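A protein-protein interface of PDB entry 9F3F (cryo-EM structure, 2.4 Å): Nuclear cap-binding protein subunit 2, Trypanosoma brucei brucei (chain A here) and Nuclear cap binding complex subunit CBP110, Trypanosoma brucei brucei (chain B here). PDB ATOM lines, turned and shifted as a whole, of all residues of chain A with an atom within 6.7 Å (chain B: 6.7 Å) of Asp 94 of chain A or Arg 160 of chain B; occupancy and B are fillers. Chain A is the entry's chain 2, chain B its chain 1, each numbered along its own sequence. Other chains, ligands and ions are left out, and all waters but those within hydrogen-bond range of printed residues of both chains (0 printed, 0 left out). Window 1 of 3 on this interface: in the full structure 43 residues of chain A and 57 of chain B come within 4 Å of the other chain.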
ATOM      1  N   ALA A   2     -11.225  11.294  22.021  1.00  0.00           N
ATOM      2  CA  ALA A   2     -11.998  12.539  21.783  1.00  0.00           C
ATOM      3  C   ALA A   2     -11.998  12.629  20.263  1.00  0.00           C
ATOM      4  O   ALA A   2     -12.703  13.483  19.708  1.00  0.00           O
ATOM      5  CB  ALA A   2     -11.422  13.761  22.443  1.00  0.00           C
ATOM      6  N   LEU A   8     -17.815  14.912  22.193  1.00  0.00           N
ATOM      7  CA  LEU A   8     -16.984  16.022  22.712  1.00  0.00           C
ATOM      8  C   LEU A   8     -17.471  17.319  22.069  1.00  0.00           C
ATOM      9  O   LEU A   8     -17.261  18.388  22.675  1.00  0.00           O
ATOM     10  CB  LEU A   8     -15.514  15.738  22.399  1.00  0.00           C
ATOM     11  CG  LEU A   8     -14.767  15.007  23.513  1.00  0.00           C
ATOM     12  CD1 LEU A   8     -14.853  15.792  24.811  1.00  0.00           C
ATOM     13  CD2 LEU A   8     -15.331  13.610  23.715  1.00  0.00           C
ATOM     14  N   THR A  42     -16.743  28.809  25.808  1.00  0.00           N
ATOM     15  CA  THR A  42     -15.786  28.462  26.891  1.00  0.00           C
ATOM     16  C   THR A  42     -16.616  28.448  28.173  1.00  0.00           C
ATOM     17  O   THR A  42     -16.037  28.497  29.261  1.00  0.00           O
ATOM     18  CB  THR A  42     -14.609  29.438  26.819  1.00  0.00           C
ATOM     19  OG1 THR A  42     -14.034  29.330  25.519  1.00  0.00           O
ATOM     20  CG2 THR A  42     -13.536  29.166  27.844  1.00  0.00           C
ATOM     21  N   CYS A  65      -9.504  22.256  36.085  1.00  0.00           N
ATOM     22  CA  CYS A  65      -9.691  22.046  34.656  1.00  0.00           C
ATOM     23  C   CYS A  65      -8.982  23.108  33.830  1.00  0.00           C
ATOM     24  O   CYS A  65      -8.428  22.803  32.769  1.00  0.00           O
ATOM     25  CB  CYS A  65     -11.183  22.041  34.319  1.00  0.00           C
ATOM     26  SG  CYS A  65     -12.197  21.060  35.433  1.00  0.00           S
ATOM     27  N   GLY A  66      -8.989  24.345  34.299  1.00  0.00           N
ATOM     28  CA  GLY A  66      -8.345  25.436  33.599  1.00  0.00           C
ATOM     29  C   GLY A  66      -8.673  26.737  34.284  1.00  0.00           C
ATOM     30  O   GLY A  66      -9.521  26.803  35.177  1.00  0.00           O
ATOM     31  N   PHE A  90     -14.529  29.816  31.303  1.00  0.00           N
ATOM     32  CA  PHE A  90     -13.113  29.518  31.378  1.00  0.00           C
ATOM     33  C   PHE A  90     -12.327  30.470  30.491  1.00  0.00           C
ATOM     34  O   PHE A  90     -12.882  31.381  29.873  1.00  0.00           O
ATOM     35  CB  PHE A  90     -12.849  28.072  30.964  1.00  0.00           C
ATOM     36  CG  PHE A  90     -13.222  27.070  32.009  1.00  0.00           C
ATOM     37  CD1 PHE A  90     -14.507  26.563  32.068  1.00  0.00           C
ATOM     38  CD2 PHE A  90     -12.300  26.651  32.945  1.00  0.00           C
ATOM     39  CE1 PHE A  90     -14.858  25.651  33.030  1.00  0.00           C
ATOM     40  CE2 PHE A  90     -12.647  25.735  33.909  1.00  0.00           C
ATOM     41  CZ  PHE A  90     -13.929  25.236  33.952  1.00  0.00           C
ATOM     42  N   GLU A  91     -11.014  30.272  30.460  1.00  0.00           N
ATOM     43  CA  GLU A  91     -10.174  31.064  29.575  1.00  0.00           C
ATOM     44  C   GLU A  91     -10.090  30.432  28.193  1.00  0.00           C
ATOM     45  O   GLU A  91     -10.137  31.134  27.177  1.00  0.00           O
ATOM     46  CB  GLU A  91      -8.789  31.219  30.194  1.00  0.00           C
ATOM     47  CG  GLU A  91      -7.798  31.981  29.354  1.00  0.00           C
ATOM     48  CD  GLU A  91      -6.517  32.257  30.104  1.00  0.00           C
ATOM     49  OE1 GLU A  91      -5.627  31.382  30.103  1.00  0.00           O
ATOM     50  OE2 GLU A  91      -6.404  33.345  30.705  1.00  0.00           O
ATOM     51  N   SER A  92      -9.975  29.110  28.138  1.00  0.00           N
ATOM     52  CA  SER A  92      -9.865  28.358  26.900  1.00  0.00           C
ATOM     53  C   SER A  92     -10.964  27.308  26.843  1.00  0.00           C
ATOM     54  O   SER A  92     -11.571  26.952  27.855  1.00  0.00           O
ATOM     55  CB  SER A  92      -8.492  27.690  26.781  1.00  0.00           C
ATOM     56  OG  SER A  92      -8.362  27.012  25.547  1.00  0.00           O
ATOM     57  N   GLN A  93     -11.195  26.750  25.655  1.00  0.00           N
ATOM     58  CA  GLN A  93     -12.237  25.701  25.519  1.00  0.00           C
ATOM     59  C   GLN A  93     -11.667  24.380  26.034  1.00  0.00           C
ATOM     60  O   GLN A  93     -12.466  23.467  26.296  1.00  0.00           O
ATOM     61  CB  GLN A  93     -12.778  25.633  24.091  1.00  0.00           C
ATOM     62  CG  GLN A  93     -13.970  24.706  23.930  1.00  0.00           C
ATOM     63  CD  GLN A  93     -14.502  24.731  22.519  1.00  0.00           C
ATOM     64  OE1 GLN A  93     -13.982  25.429  21.654  1.00  0.00           O
ATOM     65  NE2 GLN A  93     -15.550  23.963  22.278  1.00  0.00           N
ATOM     66  N   ASP A  94     -10.349  24.284  26.211  1.00  0.00           N
ATOM     67  CA  ASP A  94      -9.813  23.081  26.835  1.00  0.00           C
ATOM     68  C   ASP A  94     -10.342  22.916  28.252  1.00  0.00           C
ATOM     69  O   ASP A  94     -10.667  21.801  28.675  1.00  0.00           O
ATOM     70  CB  ASP A  94      -8.289  23.127  26.834  1.00  0.00           C
ATOM     71  CG  ASP A  94      -7.719  23.426  25.468  1.00  0.00           C
ATOM     72  OD1 ASP A  94      -8.485  23.876  24.591  1.00  0.00           O
ATOM     73  OD2 ASP A  94      -6.505  23.212  25.269  1.00  0.00           O
ATOM     74  N   GLY A  95     -10.426  24.012  29.004  1.00  0.00           N
ATOM     75  CA  GLY A  95     -10.967  23.932  30.348  1.00  0.00           C
ATOM     76  C   GLY A  95     -12.438  23.579  30.365  1.00  0.00           C
ATOM     77  O   GLY A  95     -12.881  22.768  31.182  1.00  0.00           O
ATOM     78  N   ALA A  96     -13.219  24.186  29.471  1.00  0.00           N
ATOM     79  CA  ALA A  96     -14.641  23.874  29.397  1.00  0.00           C
ATOM     80  C   ALA A  96     -14.859  22.430  28.972  1.00  0.00           C
ATOM     81  O   ALA A  96     -15.793  21.770  29.439  1.00  0.00           O
ATOM     82  CB  ALA A  96     -15.337  24.831  28.435  1.00  0.00           C
ATOM     83  N   MET A  97     -14.010  21.928  28.076  1.00  0.00           N
ATOM     84  CA  MET A  97     -14.081  20.526  27.691  1.00  0.00           C
ATOM     85  C   MET A  97     -13.764  19.619  28.871  1.00  0.00           C
ATOM     86  O   MET A  97     -14.436  18.602  29.083  1.00  0.00           O
ATOM     87  CB  MET A  97     -13.125  20.259  26.530  1.00  0.00           C
ATOM     88  CG  MET A  97     -13.701  19.386  25.437  1.00  0.00           C
ATOM     89  SD  MET A  97     -12.619  19.249  24.002  1.00  0.00           S
ATOM     90  CE  MET A  97     -11.945  20.906  23.922  1.00  0.00           C
ATOM     91  N   SER A  98     -12.740  19.969  29.651  1.00  0.00           N
ATOM     92  CA  SER A  98     -12.399  19.181  30.830  1.00  0.00           C
ATOM     93  C   SER A  98     -13.502  19.239  31.876  1.00  0.00           C
ATOM     94  O   SER A  98     -13.812  18.228  32.514  1.00  0.00           O
ATOM     95  CB  SER A  98     -11.078  19.670  31.413  1.00  0.00           C
ATOM     96  OG  SER A  98     -10.089  19.755  30.407  1.00  0.00           O
ATOM     97  N   ALA A  99     -14.097  20.414  32.075  1.00  0.00           N
ATOM     98  CA  ALA A  99     -15.149  20.551  33.073  1.00  0.00           C
ATOM     99  C   ALA A  99     -16.358  19.696  32.729  1.00  0.00           C
ATOM    100  O   ALA A  99     -16.930  19.036  33.602  1.00  0.00           O
ATOM    101  CB  ALA A  99     -15.551  22.018  33.208  1.00  0.00           C
ATOM    102  N   ILE A 101     -16.415  17.032  30.775  1.00  0.00           N
ATOM    103  CA  ILE A 101     -16.058  15.618  30.795  1.00  0.00           C
ATOM    104  C   ILE A 101     -15.778  15.151  32.218  1.00  0.00           C
ATOM    105  O   ILE A 101     -16.433  14.236  32.731  1.00  0.00           O
ATOM    106  CB  ILE A 101     -14.851  15.355  29.877  1.00  0.00           C
ATOM    107  CG1 ILE A 101     -15.239  15.539  28.411  1.00  0.00           C
ATOM    108  CG2 ILE A 101     -14.299  13.967  30.112  1.00  0.00           C
ATOM    109  CD1 ILE A 101     -16.530  14.859  28.030  1.00  0.00           C
ATOM    110  N   ASP A 102     -14.799  15.775  32.875  1.00  0.00           N
ATOM    111  CA  ASP A 102     -14.340  15.277  34.167  1.00  0.00           C
ATOM    112  C   ASP A 102     -15.322  15.596  35.286  1.00  0.00           C
ATOM    113  O   ASP A 102     -15.598  14.740  36.134  1.00  0.00           O
ATOM    114  CB  ASP A 102     -12.965  15.855  34.484  1.00  0.00           C
ATOM    115  CG  ASP A 102     -11.914  15.438  33.483  1.00  0.00           C
ATOM    116  OD1 ASP A 102     -11.384  14.316  33.609  1.00  0.00           O
ATOM    117  OD2 ASP A 102     -11.613  16.233  32.566  1.00  0.00           O
ATOM    118  N   TRP A 117     -22.749  22.235  28.583  1.00  0.00           N
ATOM    119  CA  TRP A 117     -22.125  23.243  27.692  1.00  0.00           C
ATOM    120  C   TRP A 117     -23.136  24.363  27.465  1.00  0.00           C
ATOM    121  O   TRP A 117     -24.275  24.040  27.122  1.00  0.00           O
ATOM    122  CB  TRP A 117     -21.696  22.615  26.371  1.00  0.00           C
ATOM    123  CG  TRP A 117     -20.422  21.841  26.306  1.00  0.00           C
ATOM    124  CD1 TRP A 117     -20.290  20.485  26.335  1.00  0.00           C
ATOM    125  CD2 TRP A 117     -19.105  22.368  26.084  1.00  0.00           C
ATOM    126  NE1 TRP A 117     -18.976  20.136  26.195  1.00  0.00           N
ATOM    127  CE2 TRP A 117     -18.226  21.269  26.039  1.00  0.00           C
ATOM    128  CE3 TRP A 117     -18.580  23.656  25.953  1.00  0.00           C
ATOM    129  CZ2 TRP A 117     -16.854  21.421  25.865  1.00  0.00           C
ATOM    130  CZ3 TRP A 117     -17.226  23.803  25.771  1.00  0.00           C
ATOM    131  CH2 TRP A 117     -16.376  22.701  25.732  1.00  0.00           C
ATOM    132  N   PHE B 157       0.091  14.414  16.734  1.00  0.00           N
ATOM    133  CA  PHE B 157       0.227  14.496  18.197  1.00  0.00           C
ATOM    134  C   PHE B 157      -1.161  14.572  18.813  1.00  0.00           C
ATOM    135  O   PHE B 157      -2.011  15.294  18.290  1.00  0.00           O
ATOM    136  CB  PHE B 157       1.134  15.662  18.582  1.00  0.00           C
ATOM    137  CG  PHE B 157       2.599  15.462  18.292  1.00  0.00           C
ATOM    138  CD1 PHE B 157       3.058  15.315  16.995  1.00  0.00           C
ATOM    139  CD2 PHE B 157       3.519  15.396  19.324  1.00  0.00           C
ATOM    140  CE1 PHE B 157       4.405  15.128  16.735  1.00  0.00           C
ATOM    141  CE2 PHE B 157       4.865  15.206  19.064  1.00  0.00           C
ATOM    142  CZ  PHE B 157       5.306  15.072  17.770  1.00  0.00           C
ATOM    143  N   LEU B 158      -1.369  13.836  19.893  1.00  0.00           N
ATOM    144  CA  LEU B 158      -2.680  13.835  20.574  1.00  0.00           C
ATOM    145  C   LEU B 158      -2.899  15.203  21.214  1.00  0.00           C
ATOM    146  O   LEU B 158      -1.951  15.768  21.750  1.00  0.00           O
ATOM    147  CB  LEU B 158      -2.722  12.699  21.598  1.00  0.00           C
ATOM    148  CG  LEU B 158      -2.858  11.284  21.046  1.00  0.00           C
ATOM    149  CD1 LEU B 158      -1.520  10.747  20.579  1.00  0.00           C
ATOM    150  CD2 LEU B 158      -3.457  10.357  22.089  1.00  0.00           C
ATOM    151  N   PRO B 159      -4.122  15.752  21.142  1.00  0.00           N
ATOM    152  CA  PRO B 159      -4.410  17.046  21.723  1.00  0.00           C
ATOM    153  C   PRO B 159      -4.420  17.023  23.257  1.00  0.00           C
ATOM    154  O   PRO B 159      -5.049  16.166  23.809  1.00  0.00           O
ATOM    155  CB  PRO B 159      -5.823  17.318  21.205  1.00  0.00           C
ATOM    156  CG  PRO B 159      -6.429  15.956  21.021  1.00  0.00           C
ATOM    157  CD  PRO B 159      -5.278  15.127  20.505  1.00  0.00           C
ATOM    158  N   ARG B 160      -3.793  18.017  23.879  1.00  0.00           N
ATOM    159  CA  ARG B 160      -3.972  18.405  25.304  1.00  0.00           C
ATOM    160  C   ARG B 160      -3.157  17.469  26.208  1.00  0.00           C
ATOM    161  O   ARG B 160      -3.421  17.471  27.407  1.00  0.00           O
ATOM    162  CB  ARG B 160      -5.457  18.499  25.655  1.00  0.00           C
ATOM    163  CG  ARG B 160      -6.230  19.585  24.927  1.00  0.00           C
ATOM    164  CD  ARG B 160      -7.703  19.257  25.018  1.00  0.00           C
ATOM    165  NE  ARG B 160      -8.146  19.009  26.379  1.00  0.00           N
ATOM    166  CZ  ARG B 160      -9.374  18.628  26.708  1.00  0.00           C
ATOM    167  NH1 ARG B 160     -10.223  18.252  25.770  1.00  0.00           N
ATOM    168  NH2 ARG B 160      -9.743  18.596  27.977  1.00  0.00           N
ATOM    169  N   VAL B 161      -2.222  16.679  25.661  1.00  0.00           N
ATOM    170  CA  VAL B 161      -1.369  15.864  26.577  1.00  0.00           C
ATOM    171  C   VAL B 161       0.091  15.955  26.149  1.00  0.00           C
ATOM    172  O   VAL B 161       0.355  16.163  24.947  1.00  0.00           O
ATOM    173  CB  VAL B 161      -1.781  14.381  26.670  1.00  0.00           C
ATOM    174  CG1 VAL B 161      -3.063  14.159  27.455  1.00  0.00           C
ATOM    175  CG2 VAL B 161      -1.791  13.680  25.320  1.00  0.00           C
ATOM    176  N   ALA B 162       0.991  15.801  27.113  1.00  0.00           N
ATOM    177  CA  ALA B 162       2.422  15.769  26.811  1.00  0.00           C
ATOM    178  C   ALA B 162       2.794  14.302  26.695  1.00  0.00           C
ATOM    179  O   ALA B 162       3.131  13.692  27.718  1.00  0.00           O
ATOM    180  CB  ALA B 162       3.184  16.451  27.903  1.00  0.00           C
ATOM    181  N   GLU B 163       2.716  13.768  25.488  1.00  0.00           N
ATOM    182  CA  GLU B 163       2.981  12.355  25.270  1.00  0.00           C
ATOM    183  C   GLU B 163       4.448  12.037  25.519  1.00  0.00           C
ATOM    184  O   GLU B 163       5.339  12.813  25.169  1.00  0.00           O
ATOM    185  CB  GLU B 163       2.596  11.956  23.848  1.00  0.00           C
ATOM    186  CG  GLU B 163       1.126  12.140  23.525  1.00  0.00           C
ATOM    187  CD  GLU B 163       0.909  12.848  22.204  1.00  0.00           C
ATOM    188  OE1 GLU B 163       0.525  14.036  22.219  1.00  0.00           O
ATOM    189  OE2 GLU B 163       1.123  12.215  21.148  1.00  0.00           O
ATOM    190  N   ARG B 292      -8.382  12.439  28.530  1.00  0.00           N
ATOM    191  CA  ARG B 292      -9.226  13.646  28.404  1.00  0.00           C
ATOM    192  C   ARG B 292     -10.672  13.198  28.548  1.00  0.00           C
ATOM    193  O   ARG B 292     -11.452  13.959  29.131  1.00  0.00           O
ATOM    194  CB  ARG B 292      -8.855  14.374  27.118  1.00  0.00           C
ATOM    195  CG  ARG B 292      -7.572  15.188  27.199  1.00  0.00           C
ATOM    196  CD  ARG B 292      -6.357  14.519  27.806  1.00  0.00           C
ATOM    197  NE  ARG B 292      -5.951  13.232  27.257  1.00  0.00           N
ATOM    198  CZ  ARG B 292      -5.570  13.005  26.005  1.00  0.00           C
ATOM    199  NH1 ARG B 292      -5.594  13.977  25.111  1.00  0.00           N
ATOM    200  NH2 ARG B 292      -5.145  11.804  25.655  1.00  0.00           N
ATOM    201  N   VAL B 293     -11.018  12.029  28.019  1.00  0.00           N
ATOM    202  CA  VAL B 293     -12.388  11.484  28.240  1.00  0.00           C
ATOM    203  C   VAL B 293     -12.325  10.490  29.407  1.00  0.00           C
ATOM    204  O   VAL B 293     -11.914   9.348  29.175  1.00  0.00           O
ATOM    205  CB  VAL B 293     -12.952  10.870  26.950  1.00  0.00           C
ATOM    206  CG1 VAL B 293     -14.459  10.699  27.047  1.00  0.00           C
ATOM    207  CG2 VAL B 293     -12.601  11.711  25.735  1.00  0.00           C
ATOM    208  N   TYR B 332       3.598  13.127  35.773  1.00  0.00           N
ATOM    209  CA  TYR B 332       3.114  14.107  34.812  1.00  0.00           C
ATOM    210  C   TYR B 332       3.142  15.509  35.396  1.00  0.00           C
ATOM    211  O   TYR B 332       3.598  16.451  34.738  1.00  0.00           O
ATOM    212  CB  TYR B 332       1.699  13.734  34.375  1.00  0.00           C
ATOM    213  CG  TYR B 332       1.231  14.413  33.114  1.00  0.00           C
ATOM    214  CD1 TYR B 332       1.563  13.908  31.869  1.00  0.00           C
ATOM    215  CD2 TYR B 332       0.441  15.549  33.170  1.00  0.00           C
ATOM    216  CE1 TYR B 332       1.135  14.522  30.719  1.00  0.00           C
ATOM    217  CE2 TYR B 332       0.008  16.168  32.024  1.00  0.00           C
ATOM    218  CZ  TYR B 332       0.357  15.649  30.802  1.00  0.00           C
ATOM    219  OH  TYR B 332      -0.072  16.260  29.651  1.00  0.00           O
ATOM    220  N   ASP B 338       2.394  20.484  29.172  1.00  0.00           N
ATOM    221  CA  ASP B 338       1.471  20.434  28.054  1.00  0.00           C
ATOM    222  C   ASP B 338       0.663  21.709  27.876  1.00  0.00           C
ATOM    223  O   ASP B 338      -0.034  21.839  26.865  1.00  0.00           O
ATOM    224  CB  ASP B 338       0.513  19.243  28.206  1.00  0.00           C
ATOM    225  CG  ASP B 338      -0.248  19.276  29.508  1.00  0.00           C
ATOM    226  OD1 ASP B 338       0.387  19.443  30.568  1.00  0.00           O
ATOM    227  OD2 ASP B 338      -1.479  19.106  29.472  1.00  0.00           O
ATOM    228  N   GLY B 339       0.737  22.645  28.817  1.00  0.00           N
ATOM    229  CA  GLY B 339       0.091  23.932  28.681  1.00  0.00           C
ATOM    230  C   GLY B 339      -1.414  23.869  28.557  1.00  0.00           C
ATOM    231  O   GLY B 339      -1.989  24.531  27.692  1.00  0.00           O
ATOM    232  N   THR B 340      -2.073  23.088  29.410  1.00  0.00           N
ATOM    233  CA  THR B 340      -3.517  22.950  29.332  1.00  0.00           C
ATOM    234  C   THR B 340      -4.252  23.470  30.559  1.00  0.00           C
ATOM    235  O   THR B 340      -5.464  23.692  30.481  1.00  0.00           O
ATOM    236  CB  THR B 340      -3.906  21.484  29.096  1.00  0.00           C
ATOM    237  OG1 THR B 340      -5.222  21.424  28.536  1.00  0.00           O
ATOM    238  CG2 THR B 340      -3.895  20.714  30.397  1.00  0.00           C
ATOM    239  N   ARG B 342      -5.071  21.892  33.164  1.00  0.00           N
ATOM    240  CA  ARG B 342      -5.877  20.838  33.760  1.00  0.00           C
ATOM    241  C   ARG B 342      -4.989  20.027  34.692  1.00  0.00           C
ATOM    242  O   ARG B 342      -3.933  19.539  34.278  1.00  0.00           O
ATOM    243  CB  ARG B 342      -6.494  19.951  32.679  1.00  0.00           C
ATOM    244  CG  ARG B 342      -7.201  18.715  33.188  1.00  0.00           C
ATOM    245  CD  ARG B 342      -7.979  18.039  32.070  1.00  0.00           C
ATOM    246  NE  ARG B 342      -8.003  16.586  32.189  1.00  0.00           N
ATOM    247  CZ  ARG B 342      -7.047  15.781  31.750  1.00  0.00           C
ATOM    248  NH1 ARG B 342      -5.955  16.256  31.172  1.00  0.00           N
ATOM    249  NH2 ARG B 342      -7.187  14.467  31.896  1.00  0.00           N
ATOM    250  N   SER B 947      -0.446  29.004  25.694  1.00  0.00           N
ATOM    251  CA  SER B 947      -1.241  28.166  24.804  1.00  0.00           C
ATOM    252  C   SER B 947      -2.490  28.897  24.327  1.00  0.00           C
ATOM    253  O   SER B 947      -2.841  28.833  23.143  1.00  0.00           O
ATOM    254  CB  SER B 947      -1.614  26.863  25.509  1.00  0.00           C
ATOM    255  OG  SER B 947      -0.454  26.136  25.870  1.00  0.00           O
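NH2 of Arg 160 of chain B is in hydrogen-bond range of O of Asp 94 of chain A (3.4 Å). NH1 of Arg 160 of chain B sits at hydrogen-bond distance from SD of Met 97 of chain A (3.1 Å). The guanidinium group (NH2) of Arg 160 of chain B lies within hydrogen-bond range of the side-chain hydroxyl (OG) of Ser 98 of chain A, at 2.7 Å. NE of Arg 342 of chain B is in salt-bridge range of OD2 of Asp 102 of chain A (3.6 Å).
The backbone carbonyl oxygen of Pro 159 of chain B lies within hydrogen-bond range of the guanidinium group of Arg 292 of chain B. OG of Ser 92 of chain A lies within hydrogen-bond range of OD1 of Asp 94 of chain A. The backbone carbonyl oxygen (O) of Asp 94 of chain A is in hydrogen-bond range of the side-chain hydroxyl (OG) of Ser 98 of chain A (2.7 Å).
CG2 of Val 293 of chain B touches N of Ala 2 of chain A, 3.98 Å away. Val 293 of chain B touches Leu 8 of chain A. Cys 65 of chain A touches Thr 340 of chain B (O to O, 3.8 Å). O of Cys 65 of chain A touches CA of Arg 342 of chain B, at 3.4 Å. Asp 94 of chain A touches Thr 340 of chain B. OG of Ser 98 of chain A touches CD of Arg 342 of chain B, 3.2 Å away. Arg 292 of chain B touches Ile 101 of chain A (O to CG2, 3.0 Å). Ile 101 of chain A touches Val 293 of chain B (CG2 to CA, 3.6 Å).
Of the printed residues of chain B, Ile 101 of chain A touches Arg 292 and Val 293. Printed residues of chain B within 4 Å of Ser 98 of chain A: Arg 160 and Arg 342. Printed residues of chain A within 4 Å of Arg 292 of chain B: Ile 101 (3.0 Å). Of the printed residues of chain A, Val 293 of chain B touches Ala 2, Leu 8 and Ile 101. Of the printed residues of chain B, Ala 2 of chain A touches Val 293 (3.98 Å). The nearest residue of chain A that does not touch Arg 160 of chain B is Leu 8 of chain A (5.3 Å).
Hydrophobic or aromatic side chains of chain B that line the printed part of chain A: Val 293. Printed residues of chain A that touch a printed residue of chain B: Ala 2, Leu 8, Cys 65, Asp 94, Met 97, Ser 98, Ile 101 and Asp 102. Along chain A the printed residues that touch a printed residue of chain B span positions 2 to 102. Among the printed residues, Asp or Glu carboxylates within 4 Å of a Lys or Arg side-chain nitrogen of the other chain: Asp 102 of chain A with Arg 342 of chain B.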
